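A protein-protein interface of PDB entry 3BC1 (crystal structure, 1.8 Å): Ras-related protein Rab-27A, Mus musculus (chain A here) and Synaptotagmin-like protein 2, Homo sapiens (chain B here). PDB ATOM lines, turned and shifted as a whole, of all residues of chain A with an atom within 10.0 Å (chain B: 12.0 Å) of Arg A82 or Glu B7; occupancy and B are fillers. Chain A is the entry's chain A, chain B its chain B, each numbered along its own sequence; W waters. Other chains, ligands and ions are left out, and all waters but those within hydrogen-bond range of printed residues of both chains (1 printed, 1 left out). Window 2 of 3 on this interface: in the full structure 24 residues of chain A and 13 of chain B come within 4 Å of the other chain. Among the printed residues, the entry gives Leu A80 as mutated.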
ATOM      1  N   SER A  20     -22.371 -35.628   9.303  1.00  0.00           N
ATOM      2  CA  SER A  20     -22.557 -36.295  10.589  1.00  0.00           C
ATOM      3  C   SER A  20     -21.591 -37.473  10.694  1.00  0.00           C
ATOM      4  O   SER A  20     -21.431 -38.233   9.744  1.00  0.00           O
ATOM      5  CB  SER A  20     -23.992 -36.791  10.761  1.00  0.00           C
ATOM      6  OG  SER A  20     -24.172 -37.370  12.047  1.00  0.00           O
ATOM      7  N   THR A  42     -24.155 -37.868  19.063  1.00  0.00           N
ATOM      8  CA  THR A  42     -24.405 -36.913  17.985  1.00  0.00           C
ATOM      9  C   THR A  42     -24.824 -35.554  18.551  1.00  0.00           C
ATOM     10  O   THR A  42     -25.517 -35.469  19.571  1.00  0.00           O
ATOM     11  CB  THR A  42     -25.445 -37.449  16.965  1.00  0.00           C
ATOM     12  OG1 THR A  42     -25.440 -36.636  15.778  1.00  0.00           O
ATOM     13  CG2 THR A  42     -26.853 -37.502  17.572  1.00  0.00           C
ATOM     14  N   THR A  43     -24.378 -34.496  17.887  1.00  0.00           N
ATOM     15  CA  THR A  43     -24.535 -33.147  18.397  1.00  0.00           C
ATOM     16  C   THR A  43     -25.965 -32.671  18.161  1.00  0.00           C
ATOM     17  O   THR A  43     -26.501 -32.807  17.056  1.00  0.00           O
ATOM     18  CB  THR A  43     -23.525 -32.176  17.741  1.00  0.00           C
ATOM     19  OG1 THR A  43     -22.182 -32.582  18.069  1.00  0.00           O
ATOM     20  CG2 THR A  43     -23.757 -30.745  18.204  1.00  0.00           C
ATOM     21  N   VAL A  44     -26.567 -32.126  19.214  1.00  0.00           N
ATOM     22  CA  VAL A  44     -27.944 -31.648  19.165  1.00  0.00           C
ATOM     23  C   VAL A  44     -27.933 -30.230  18.617  1.00  0.00           C
ATOM     24  O   VAL A  44     -27.917 -29.257  19.363  1.00  0.00           O
ATOM     25  CB  VAL A  44     -28.621 -31.727  20.559  1.00  0.00           C
ATOM     26  CG1 VAL A  44     -30.044 -31.182  20.514  1.00  0.00           C
ATOM     27  CG2 VAL A  44     -28.638 -33.164  21.056  1.00  0.00           C
ATOM     28  N   GLY A  45     -27.912 -30.131  17.289  1.00  0.00           N
ATOM     29  CA  GLY A  45     -27.965 -28.844  16.596  1.00  0.00           C
ATOM     30  C   GLY A  45     -26.635 -28.123  16.571  1.00  0.00           C
ATOM     31  O   GLY A  45     -25.972 -28.057  15.531  1.00  0.00           O
ATOM     32  N   ILE A  46     -26.241 -27.578  17.718  1.00  0.00           N
ATOM     33  CA  ILE A  46     -25.027 -26.782  17.792  1.00  0.00           C
ATOM     34  C   ILE A  46     -24.443 -26.809  19.204  1.00  0.00           C
ATOM     35  O   ILE A  46     -25.165 -26.995  20.188  1.00  0.00           O
ATOM     36  CB  ILE A  46     -25.314 -25.327  17.327  1.00  0.00           C
ATOM     37  CG1 ILE A  46     -24.025 -24.607  16.911  1.00  0.00           C
ATOM     38  CG2 ILE A  46     -26.076 -24.560  18.408  1.00  0.00           C
ATOM     39  CD1 ILE A  46     -24.178 -23.769  15.656  1.00  0.00           C
ATOM     40  N   ASP A  47     -23.128 -26.635  19.285  1.00  0.00           N
ATOM     41  CA  ASP A  47     -22.431 -26.509  20.558  1.00  0.00           C
ATOM     42  C   ASP A  47     -21.135 -25.732  20.301  1.00  0.00           C
ATOM     43  O   ASP A  47     -20.792 -25.474  19.149  1.00  0.00           O
ATOM     44  CB  ASP A  47     -22.140 -27.903  21.121  1.00  0.00           C
ATOM     45  CG  ASP A  47     -21.772 -27.891  22.602  1.00  0.00           C
ATOM     46  OD1 ASP A  47     -21.787 -26.819  23.243  1.00  0.00           O
ATOM     47  OD2 ASP A  47     -21.451 -28.983  23.122  1.00  0.00           O
ATOM     48  N   ALA A  78     -23.813 -29.454  14.102  1.00  0.00           N
ATOM     49  CA  ALA A  78     -24.314 -30.789  13.767  1.00  0.00           C
ATOM     50  C   ALA A  78     -24.319 -30.989  12.250  1.00  0.00           C
ATOM     51  O   ALA A  78     -24.585 -30.051  11.489  1.00  0.00           O
ATOM     52  CB  ALA A  78     -25.720 -31.004  14.336  1.00  0.00           C
ATOM     53  N   GLY A  79     -24.022 -32.216  11.825  1.00  0.00           N
ATOM     54  CA  GLY A  79     -23.933 -32.564  10.414  1.00  0.00           C
ATOM     55  C   GLY A  79     -25.233 -33.035   9.784  1.00  0.00           C
ATOM     56  O   GLY A  79     -25.384 -32.972   8.565  1.00  0.00           O
ATOM     57  N   LEU A  80     -26.165 -33.526  10.597  1.00  0.00           N
ATOM     58  CA  LEU A  80     -27.435 -34.021  10.080  1.00  0.00           C
ATOM     59  C   LEU A  80     -28.275 -32.882   9.492  1.00  0.00           C
ATOM     60  O   LEU A  80     -28.358 -31.794  10.070  1.00  0.00           O
ATOM     61  CB  LEU A  80     -28.234 -34.730  11.170  1.00  0.00           C
ATOM     62  CG  LEU A  80     -27.704 -36.073  11.651  1.00  0.00           C
ATOM     63  CD1 LEU A  80     -28.665 -36.624  12.688  1.00  0.00           C
ATOM     64  CD2 LEU A  80     -27.515 -37.049  10.499  1.00  0.00           C
ATOM     65  N   GLU A  81     -28.921 -33.168   8.363  1.00  0.00           N
ATOM     66  CA  GLU A  81     -29.626 -32.155   7.574  1.00  0.00           C
ATOM     67  C   GLU A  81     -30.824 -31.544   8.291  1.00  0.00           C
ATOM     68  O   GLU A  81     -31.276 -30.464   7.923  1.00  0.00           O
ATOM     69  CB  GLU A  81     -30.061 -32.732   6.219  1.00  0.00           C
ATOM     70  CG  GLU A  81     -28.888 -33.100   5.325  1.00  0.00           C
ATOM     71  CD  GLU A  81     -29.284 -33.467   3.908  1.00  0.00           C
ATOM     72  OE1 GLU A  81     -28.429 -34.043   3.196  1.00  0.00           O
ATOM     73  OE2 GLU A  81     -30.430 -33.172   3.491  1.00  0.00           O
ATOM     74  N   ARG A  82     -31.335 -32.223   9.313  1.00  0.00           N
ATOM     75  CA  ARG A  82     -32.412 -31.673  10.139  1.00  0.00           C
ATOM     76  C   ARG A  82     -31.987 -30.413  10.905  1.00  0.00           C
ATOM     77  O   ARG A  82     -32.833 -29.616  11.308  1.00  0.00           O
ATOM     78  CB  ARG A  82     -32.918 -32.733  11.120  1.00  0.00           C
ATOM     79  CG  ARG A  82     -31.890 -33.158  12.158  1.00  0.00           C
ATOM     80  CD  ARG A  82     -32.079 -34.608  12.566  1.00  0.00           C
ATOM     81  NE  ARG A  82     -33.402 -34.834  13.138  1.00  0.00           N
ATOM     82  CZ  ARG A  82     -33.779 -34.430  14.347  1.00  0.00           C
ATOM     83  NH1 ARG A  82     -32.931 -33.777  15.127  1.00  0.00           N
ATOM     84  NH2 ARG A  82     -35.011 -34.682  14.786  1.00  0.00           N
ATOM     85  N   PHE A  83     -30.679 -30.250  11.108  1.00  0.00           N
ATOM     86  CA  PHE A  83     -30.121 -29.064  11.761  1.00  0.00           C
ATOM     87  C   PHE A  83     -29.446 -28.097  10.779  1.00  0.00           C
ATOM     88  O   PHE A  83     -28.747 -27.174  11.200  1.00  0.00           O
ATOM     89  CB  PHE A  83     -29.107 -29.493  12.830  1.00  0.00           C
ATOM     90  CG  PHE A  83     -29.709 -30.280  13.963  1.00  0.00           C
ATOM     91  CD1 PHE A  83     -30.676 -29.710  14.777  1.00  0.00           C
ATOM     92  CD2 PHE A  83     -29.293 -31.584  14.231  1.00  0.00           C
ATOM     93  CE1 PHE A  83     -31.234 -30.424  15.833  1.00  0.00           C
ATOM     94  CE2 PHE A  83     -29.843 -32.303  15.291  1.00  0.00           C
ATOM     95  CZ  PHE A  83     -30.812 -31.717  16.095  1.00  0.00           C
ATOM     96  N   ARG A  84     -29.656 -28.289   9.480  1.00  0.00           N
ATOM     97  CA  ARG A  84     -28.867 -27.558   8.485  1.00  0.00           C
ATOM     98  C   ARG A  84     -29.147 -26.062   8.477  1.00  0.00           C
ATOM     99  O   ARG A  84     -28.227 -25.271   8.278  1.00  0.00           O
ATOM    100  CB  ARG A  84     -29.075 -28.123   7.080  1.00  0.00           C
ATOM    101  CG  ARG A  84     -28.104 -27.572   6.024  1.00  0.00           C
ATOM    102  CD  ARG A  84     -26.629 -27.827   6.362  1.00  0.00           C
ATOM    103  NE  ARG A  84     -26.339 -29.239   6.625  1.00  0.00           N
ATOM    104  CZ  ARG A  84     -26.219 -30.177   5.685  1.00  0.00           C
ATOM    105  NH1 ARG A  84     -26.352 -29.882   4.399  1.00  0.00           N
ATOM    106  NH2 ARG A  84     -25.955 -31.427   6.033  1.00  0.00           N
ATOM    107  N   SER A  85     -30.403 -25.670   8.682  1.00  0.00           N
ATOM    108  CA  SER A  85     -30.746 -24.246   8.713  1.00  0.00           C
ATOM    109  C   SER A  85     -30.148 -23.564   9.949  1.00  0.00           C
ATOM    110  O   SER A  85     -29.597 -22.466   9.846  1.00  0.00           O
ATOM    111  CB  SER A  85     -32.262 -24.022   8.633  1.00  0.00           C
ATOM    112  OG  SER A  85     -32.903 -24.298   9.868  1.00  0.00           O
ATOM    113  N   LEU A  86     -30.237 -24.222  11.103  1.00  0.00           N
ATOM    114  CA  LEU A  86     -29.613 -23.706  12.322  1.00  0.00           C
ATOM    115  C   LEU A  86     -28.110 -23.525  12.135  1.00  0.00           C
ATOM    116  O   LEU A  86     -27.578 -22.457  12.413  1.00  0.00           O
ATOM    117  CB  LEU A  86     -29.876 -24.622  13.523  1.00  0.00           C
ATOM    118  CG  LEU A  86     -29.313 -24.130  14.866  1.00  0.00           C
ATOM    119  CD1 LEU A  86     -29.931 -22.792  15.285  1.00  0.00           C
ATOM    120  CD2 LEU A  86     -29.509 -25.171  15.964  1.00  0.00           C
ATOM    121  N   THR A  87     -27.430 -24.561  11.653  1.00  0.00           N
ATOM    122  CA  THR A  87     -25.977 -24.510  11.524  1.00  0.00           C
ATOM    123  C   THR A  87     -25.547 -23.498  10.456  1.00  0.00           C
ATOM    124  O   THR A  87     -24.550 -22.801  10.636  1.00  0.00           O
ATOM    125  CB  THR A  87     -25.360 -25.897  11.232  1.00  0.00           C
ATOM    126  OG1 THR A  87     -25.856 -26.401   9.991  1.00  0.00           O
ATOM    127  CG2 THR A  87     -25.692 -26.890  12.349  1.00  0.00           C
ATOM    128  N   THR A  88     -26.298 -23.402   9.360  1.00  0.00           N
ATOM    129  CA  THR A  88     -25.987 -22.407   8.320  1.00  0.00           C
ATOM    130  C   THR A  88     -26.106 -20.985   8.863  1.00  0.00           C
ATOM    131  O   THR A  88     -25.289 -20.123   8.536  1.00  0.00           O
ATOM    132  CB  THR A  88     -26.895 -22.551   7.083  1.00  0.00           C
ATOM    133  OG1 THR A  88     -26.736 -23.864   6.530  1.00  0.00           O
ATOM    134  CG2 THR A  88     -26.527 -21.517   6.020  1.00  0.00           C
ATOM    135  N   TRP A 115     -20.069 -28.519   0.783  1.00  0.00           N
ATOM    136  CA  TRP A 115     -19.856 -27.708   1.981  1.00  0.00           C
ATOM    137  C   TRP A 115     -19.135 -26.401   1.645  1.00  0.00           C
ATOM    138  O   TRP A 115     -19.502 -25.344   2.148  1.00  0.00           O
ATOM    139  CB  TRP A 115     -19.054 -28.469   3.039  1.00  0.00           C
ATOM    140  CG  TRP A 115     -19.821 -29.531   3.762  1.00  0.00           C
ATOM    141  CD1 TRP A 115     -19.627 -30.877   3.677  1.00  0.00           C
ATOM    142  CD2 TRP A 115     -20.881 -29.336   4.708  1.00  0.00           C
ATOM    143  NE1 TRP A 115     -20.501 -31.533   4.502  1.00  0.00           N
ATOM    144  CE2 TRP A 115     -21.284 -30.613   5.148  1.00  0.00           C
ATOM    145  CE3 TRP A 115     -21.529 -28.207   5.224  1.00  0.00           C
ATOM    146  CZ2 TRP A 115     -22.309 -30.795   6.075  1.00  0.00           C
ATOM    147  CZ3 TRP A 115     -22.543 -28.386   6.150  1.00  0.00           C
ATOM    148  CH2 TRP A 115     -22.928 -29.673   6.562  1.00  0.00           C
ATOM    149  N   GLY B   1     -39.877 -34.033  28.791  1.00  0.00           N
ATOM    150  CA  GLY B   1     -40.400 -33.346  27.577  1.00  0.00           C
ATOM    151  C   GLY B   1     -40.314 -34.223  26.347  1.00  0.00           C
ATOM    152  O   GLY B   1     -39.686 -35.282  26.374  1.00  0.00           O
ATOM    153  N   SER B   2     -40.945 -33.782  25.259  1.00  0.00           N
ATOM    154  CA  SER B   2     -40.814 -34.479  23.984  1.00  0.00           C
ATOM    155  C   SER B   2     -39.374 -34.332  23.484  1.00  0.00           C
ATOM    156  O   SER B   2     -38.637 -33.460  23.959  1.00  0.00           O
ATOM    157  CB  SER B   2     -41.810 -33.939  22.947  1.00  0.00           C
ATOM    158  OG  SER B   2     -41.533 -32.590  22.598  1.00  0.00           O
ATOM    159  N   PRO B   3     -38.948 -35.211  22.559  1.00  0.00           N
ATOM    160  CA  PRO B   3     -37.641 -35.009  21.938  1.00  0.00           C
ATOM    161  C   PRO B   3     -37.526 -33.635  21.271  1.00  0.00           C
ATOM    162  O   PRO B   3     -36.529 -32.947  21.477  1.00  0.00           O
ATOM    163  CB  PRO B   3     -37.556 -36.144  20.910  1.00  0.00           C
ATOM    164  CG  PRO B   3     -38.475 -37.189  21.422  1.00  0.00           C
ATOM    165  CD  PRO B   3     -39.603 -36.439  22.071  1.00  0.00           C
ATOM    166  N   GLU B   4     -38.545 -33.242  20.502  1.00  0.00           N
ATOM    167  CA  GLU B   4     -38.619 -31.891  19.922  1.00  0.00           C
ATOM    168  C   GLU B   4     -38.255 -30.815  20.942  1.00  0.00           C
ATOM    169  O   GLU B   4     -37.398 -29.964  20.696  1.00  0.00           O
ATOM    170  CB  GLU B   4     -40.031 -31.591  19.384  1.00  0.00           C
ATOM    171  CG  GLU B   4     -40.107 -31.329  17.881  1.00  0.00           C
ATOM    172  CD  GLU B   4     -41.399 -30.621  17.462  1.00  0.00           C
ATOM    173  OE1 GLU B   4     -42.156 -30.136  18.338  1.00  0.00           O
ATOM    174  OE2 GLU B   4     -41.654 -30.545  16.244  1.00  0.00           O
ATOM    175  N   PHE B   5     -38.918 -30.863  22.090  1.00  0.00           N
ATOM    176  CA  PHE B   5     -38.723 -29.864  23.127  1.00  0.00           C
ATOM    177  C   PHE B   5     -37.346 -29.975  23.778  1.00  0.00           C
ATOM    178  O   PHE B   5     -36.675 -28.962  23.990  1.00  0.00           O
ATOM    179  CB  PHE B   5     -39.810 -29.985  24.185  1.00  0.00           C
ATOM    180  CG  PHE B   5     -39.612 -29.076  25.346  1.00  0.00           C
ATOM    181  CD1 PHE B   5     -39.733 -27.702  25.193  1.00  0.00           C
ATOM    182  CD2 PHE B   5     -39.287 -29.585  26.587  1.00  0.00           C
ATOM    183  CE1 PHE B   5     -39.542 -26.854  26.266  1.00  0.00           C
ATOM    184  CE2 PHE B   5     -39.097 -28.742  27.669  1.00  0.00           C
ATOM    185  CZ  PHE B   5     -39.220 -27.376  27.507  1.00  0.00           C
ATOM    186  N   GLU B   6     -36.931 -31.201  24.101  1.00  0.00           N
ATOM    187  CA  GLU B   6     -35.602 -31.434  24.685  1.00  0.00           C
ATOM    188  C   GLU B   6     -34.482 -30.904  23.789  1.00  0.00           C
ATOM    189  O   GLU B   6     -33.478 -30.389  24.284  1.00  0.00           O
ATOM    190  CB  GLU B   6     -35.375 -32.922  24.974  1.00  0.00           C
ATOM    191  CG  GLU B   6     -35.979 -33.402  26.291  1.00  0.00           C
ATOM    192  CD  GLU B   6     -35.652 -34.855  26.599  1.00  0.00           C
ATOM    193  OE1 GLU B   6     -34.670 -35.397  26.033  1.00  0.00           O
ATOM    194  OE2 GLU B   6     -36.387 -35.462  27.409  1.00  0.00           O
ATOM    195  N   GLU B   7     -34.654 -31.034  22.476  1.00  0.00           N
ATOM    196  CA  GLU B   7     -33.669 -30.506  21.533  1.00  0.00           C
ATOM    197  C   GLU B   7     -33.551 -28.990  21.630  1.00  0.00           C
ATOM    198  O   GLU B   7     -32.441 -28.458  21.663  1.00  0.00           O
ATOM    199  CB  GLU B   7     -33.998 -30.915  20.099  1.00  0.00           C
ATOM    200  CG  GLU B   7     -33.886 -32.401  19.867  1.00  0.00           C
ATOM    201  CD  GLU B   7     -33.763 -32.762  18.406  1.00  0.00           C
ATOM    202  OE1 GLU B   7     -34.274 -32.008  17.547  1.00  0.00           O
ATOM    203  OE2 GLU B   7     -33.146 -33.809  18.128  1.00  0.00           O
ATOM    204  N   GLN B   8     -34.690 -28.299  21.692  1.00  0.00           N
ATOM    205  CA  GLN B   8     -34.682 -26.837  21.819  1.00  0.00           C
ATOM    206  C   GLN B   8     -34.074 -26.409  23.150  1.00  0.00           C
ATOM    207  O   GLN B   8     -33.294 -25.455  23.198  1.00  0.00           O
ATOM    208  CB  GLN B   8     -36.092 -26.251  21.665  1.00  0.00           C
ATOM    209  CG  GLN B   8     -36.719 -26.480  20.291  1.00  0.00           C
ATOM    210  CD  GLN B   8     -35.843 -25.997  19.146  1.00  0.00           C
ATOM    211  OE1 GLN B   8     -35.423 -26.777  18.276  1.00  0.00           O
ATOM    212  NE2 GLN B   8     -35.550 -24.718  19.148  1.00  0.00           N
ATOM    213  N   GLU B   9     -34.426 -27.118  24.221  1.00  0.00           N
ATOM    214  CA  GLU B   9     -33.850 -26.874  25.543  1.00  0.00           C
ATOM    215  C   GLU B   9     -32.324 -26.939  25.520  1.00  0.00           C
ATOM    216  O   GLU B   9     -31.647 -26.085  26.088  1.00  0.00           O
ATOM    217  CB  GLU B   9     -34.343 -27.913  26.552  1.00  0.00           C
ATOM    218  CG  GLU B   9     -35.738 -27.697  27.073  1.00  0.00           C
ATOM    219  CD  GLU B   9     -35.953 -28.401  28.401  1.00  0.00           C
ATOM    220  OE1 GLU B   9     -35.286 -29.435  28.644  1.00  0.00           O
ATOM    221  OE2 GLU B   9     -36.771 -27.911  29.207  1.00  0.00           O
ATOM    222  N   ALA B  10     -31.795 -27.971  24.875  1.00  0.00           N
ATOM    223  CA  ALA B  10     -30.347 -28.165  24.802  1.00  0.00           C
ATOM    224  C   ALA B  10     -29.681 -27.033  24.023  1.00  0.00           C
ATOM    225  O   ALA B  10     -28.667 -26.492  24.461  1.00  0.00           O
ATOM    226  CB  ALA B  10     -30.023 -29.513  24.164  1.00  0.00           C
ATOM    227  N   ILE B  11     -30.252 -26.673  22.875  1.00  0.00           N
ATOM    228  CA  ILE B  11     -29.697 -25.586  22.066  1.00  0.00           C
ATOM    229  C   ILE B  11     -29.795 -24.241  22.809  1.00  0.00           C
ATOM    230  O   ILE B  11     -28.873 -23.426  22.758  1.00  0.00           O
ATOM    231  CB  ILE B  11     -30.376 -25.477  20.688  1.00  0.00           C
ATOM    232  CG1 ILE B  11     -30.224 -26.789  19.911  1.00  0.00           C
ATOM    233  CG2 ILE B  11     -29.762 -24.323  19.898  1.00  0.00           C
ATOM    234  CD1 ILE B  11     -31.221 -26.962  18.776  1.00  0.00           C
ATOM    235  N   MET B  12     -30.895 -24.023  23.521  1.00  0.00           N
ATOM    236  CA  MET B  12     -31.045 -22.803  24.318  1.00  0.00           C
ATOM    237  C   MET B  12     -29.932 -22.656  25.362  1.00  0.00           C
ATOM    238  O   MET B  12     -29.420 -21.561  25.566  1.00  0.00           O
ATOM    239  CB  MET B  12     -32.416 -22.749  24.996  1.00  0.00           C
ATOM    240  CG  MET B  12     -33.584 -22.468  24.052  1.00  0.00           C
ATOM    241  SD  MET B  12     -33.514 -20.872  23.213  1.00  0.00           S
ATOM    242  CE  MET B  12     -33.728 -19.753  24.597  1.00  0.00           C
ATOM    243  N   LYS B  13     -29.556 -23.756  26.010  1.00  0.00           N
ATOM    244  CA  LYS B  13     -28.461 -23.736  26.986  1.00  0.00           C
ATOM    245  C   LYS B  13     -27.137 -23.311  26.338  1.00  0.00           C
ATOM    246  O   LYS B  13     -26.354 -22.585  26.953  1.00  0.00           O
ATOM    247  CB  LYS B  13     -28.325 -25.102  27.674  1.00  0.00           C
ATOM    248  CG  LYS B  13     -29.522 -25.441  28.571  1.00  0.00           C
ATOM    249  CD  LYS B  13     -29.439 -26.833  29.177  1.00  0.00           C
ATOM    250  CE  LYS B  13     -30.622 -27.092  30.120  1.00  0.00           C
ATOM    251  NZ  LYS B  13     -30.520 -28.409  30.814  1.00  0.00           N
ATOM    252  N   VAL B  14     -26.897 -23.758  25.108  1.00  0.00           N
ATOM    253  CA  VAL B  14     -25.711 -23.335  24.342  1.00  0.00           C
ATOM    254  C   VAL B  14     -25.790 -21.829  24.057  1.00  0.00           C
ATOM    255  O   VAL B  14     -24.825 -21.090  24.269  1.00  0.00           O
ATOM    256  CB  VAL B  14     -25.565 -24.142  23.021  1.00  0.00           C
ATOM    257  CG1 VAL B  14     -24.431 -23.588  22.138  1.00  0.00           C
ATOM    258  CG2 VAL B  14     -25.313 -25.611  23.333  1.00  0.00           C
ATOM    259  N   LEU B  15     -26.950 -21.377  23.595  1.00  0.00           N
ATOM    260  CA  LEU B  15     -27.128 -19.966  23.286  1.00  0.00           C
ATOM    261  C   LEU B  15     -26.964 -19.104  24.545  1.00  0.00           C
ATOM    262  O   LEU B  15     -26.455 -17.995  24.467  1.00  0.00           O
ATOM    263  CB  LEU B  15     -28.487 -19.721  22.634  1.00  0.00           C
ATOM    264  CG  LEU B  15     -28.692 -20.350  21.251  1.00  0.00           C
ATOM    265  CD1 LEU B  15     -30.082 -20.025  20.747  1.00  0.00           C
ATOM    266  CD2 LEU B  15     -27.632 -19.878  20.258  1.00  0.00           C
ATOM    267  N   GLN B  16     -27.381 -19.623  25.697  1.00  0.00           N
ATOM    268  CA  GLN B  16     -27.231 -18.894  26.956  1.00  0.00           C
ATOM    269  C   GLN B  16     -25.761 -18.764  27.340  1.00  0.00           C
ATOM    270  O   GLN B  16     -25.326 -17.701  27.773  1.00  0.00           O
ATOM    271  CB  GLN B  16     -28.044 -19.554  28.068  1.00  0.00           C
ATOM    272  CG  GLN B  16     -29.532 -19.263  27.929  1.00  0.00           C
ATOM    273  CD  GLN B  16     -30.451 -20.334  28.489  1.00  0.00           C
ATOM    274  OE1 GLN B  16     -30.025 -21.249  29.203  1.00  0.00           O
ATOM    275  NE2 GLN B  16     -31.734 -20.218  28.163  1.00  0.00           N
ATOM    276  N   ARG B  17     -25.000 -19.838  27.154  1.00  0.00           N
ATOM    277  CA  ARG B  17     -23.561 -19.812  27.407  1.00  0.00           C
ATOM    278  C   ARG B  17     -22.834 -18.840  26.479  1.00  0.00           C
ATOM    279  O   ARG B  17     -21.916 -18.140  26.906  1.00  0.00           O
ATOM    280  CB  ARG B  17     -22.969 -21.210  27.244  1.00  0.00           C
ATOM    281  CG  ARG B  17     -23.350 -22.191  28.352  1.00  0.00           C
ATOM    282  CD  ARG B  17     -23.088 -23.629  27.931  1.00  0.00           C
ATOM    283  NE  ARG B  17     -21.772 -23.775  27.316  1.00  0.00           N
ATOM    284  CZ  ARG B  17     -21.491 -24.547  26.266  1.00  0.00           C
ATOM    285  NH1 ARG B  17     -22.426 -25.276  25.666  1.00  0.00           N
ATOM    286  NH2 ARG B  17     -20.255 -24.577  25.799  1.00  0.00           N
HETATM  287  O   HOH W   1     -19.417 -27.921  25.223  1.00  0.00           O
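Water W1 lies within hydrogen-bond range of the side-chain carboxylate of Asp A47 and the guanidinium group of Arg B17.
Among the printed residues, merely in contact across the chains: Val A44 with Glu B7 (3.8 Å), Val A44 with Ile B11 (3.4 Å), Ile A46 with Ile B11 (3.98 Å), Ile A46 with Val B14 (3.4 Å), Asp A47 with Val B14 (3.7 Å), Phe A83 with Glu B7 (3.7 Å) and Leu A86 with Ile B11 (3.7 Å).
No residue of chain B comes within 4 Å of Gly A45. Printed residues of chain B within 4 Å of Asp A47: Val B14 and Arg B17. No residue of chain B comes within 4 Å of Gly A79. No residue of chain B comes within 4 Å of Leu A80. Of chain B, only Glu B7 comes within 4 Å of Arg A82. Pro B3 touches none of the printed residues of chain A. Glu B7 touches just these residues of chain A: Val A44 (3.8 Å), Arg A82 (3.0 Å) and Phe A83 (3.7 Å). No residue of chain A comes within 4 Å of Gln B8. Printed residues of chain A within 4 Å of Val B14: Ile A46 (3.4 Å) and Asp A47 (3.7 Å).
The backbone carbonyl oxygen (O) of Phe A83 sits at hydrogen-bond distance from the side-chain hydroxyl (OG1) of Thr A87 (3.2 Å).
Hydrophobic or aromatic side chains of chain A within 4 Å of the printed part of chain B: Val A44, Ile A46, Phe A83 and Leu A86. Of the 17 printed residues of chain B, 4 touch a printed residue of chain A. Hydrophobic or aromatic side chains of chain B that line the printed part of chain A: Ile B11 and Val B14. Among the printed residues, 9 pairs touch across the chains.
The guanidinium group (NH1) of Arg A82 is in salt-bridge range of the side-chain carboxylate (OE2) of Glu B7 (3.0 Å). OD1 of Asp A47 is in salt-bridge range of NH1 of Arg B17 (2.9 Å).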
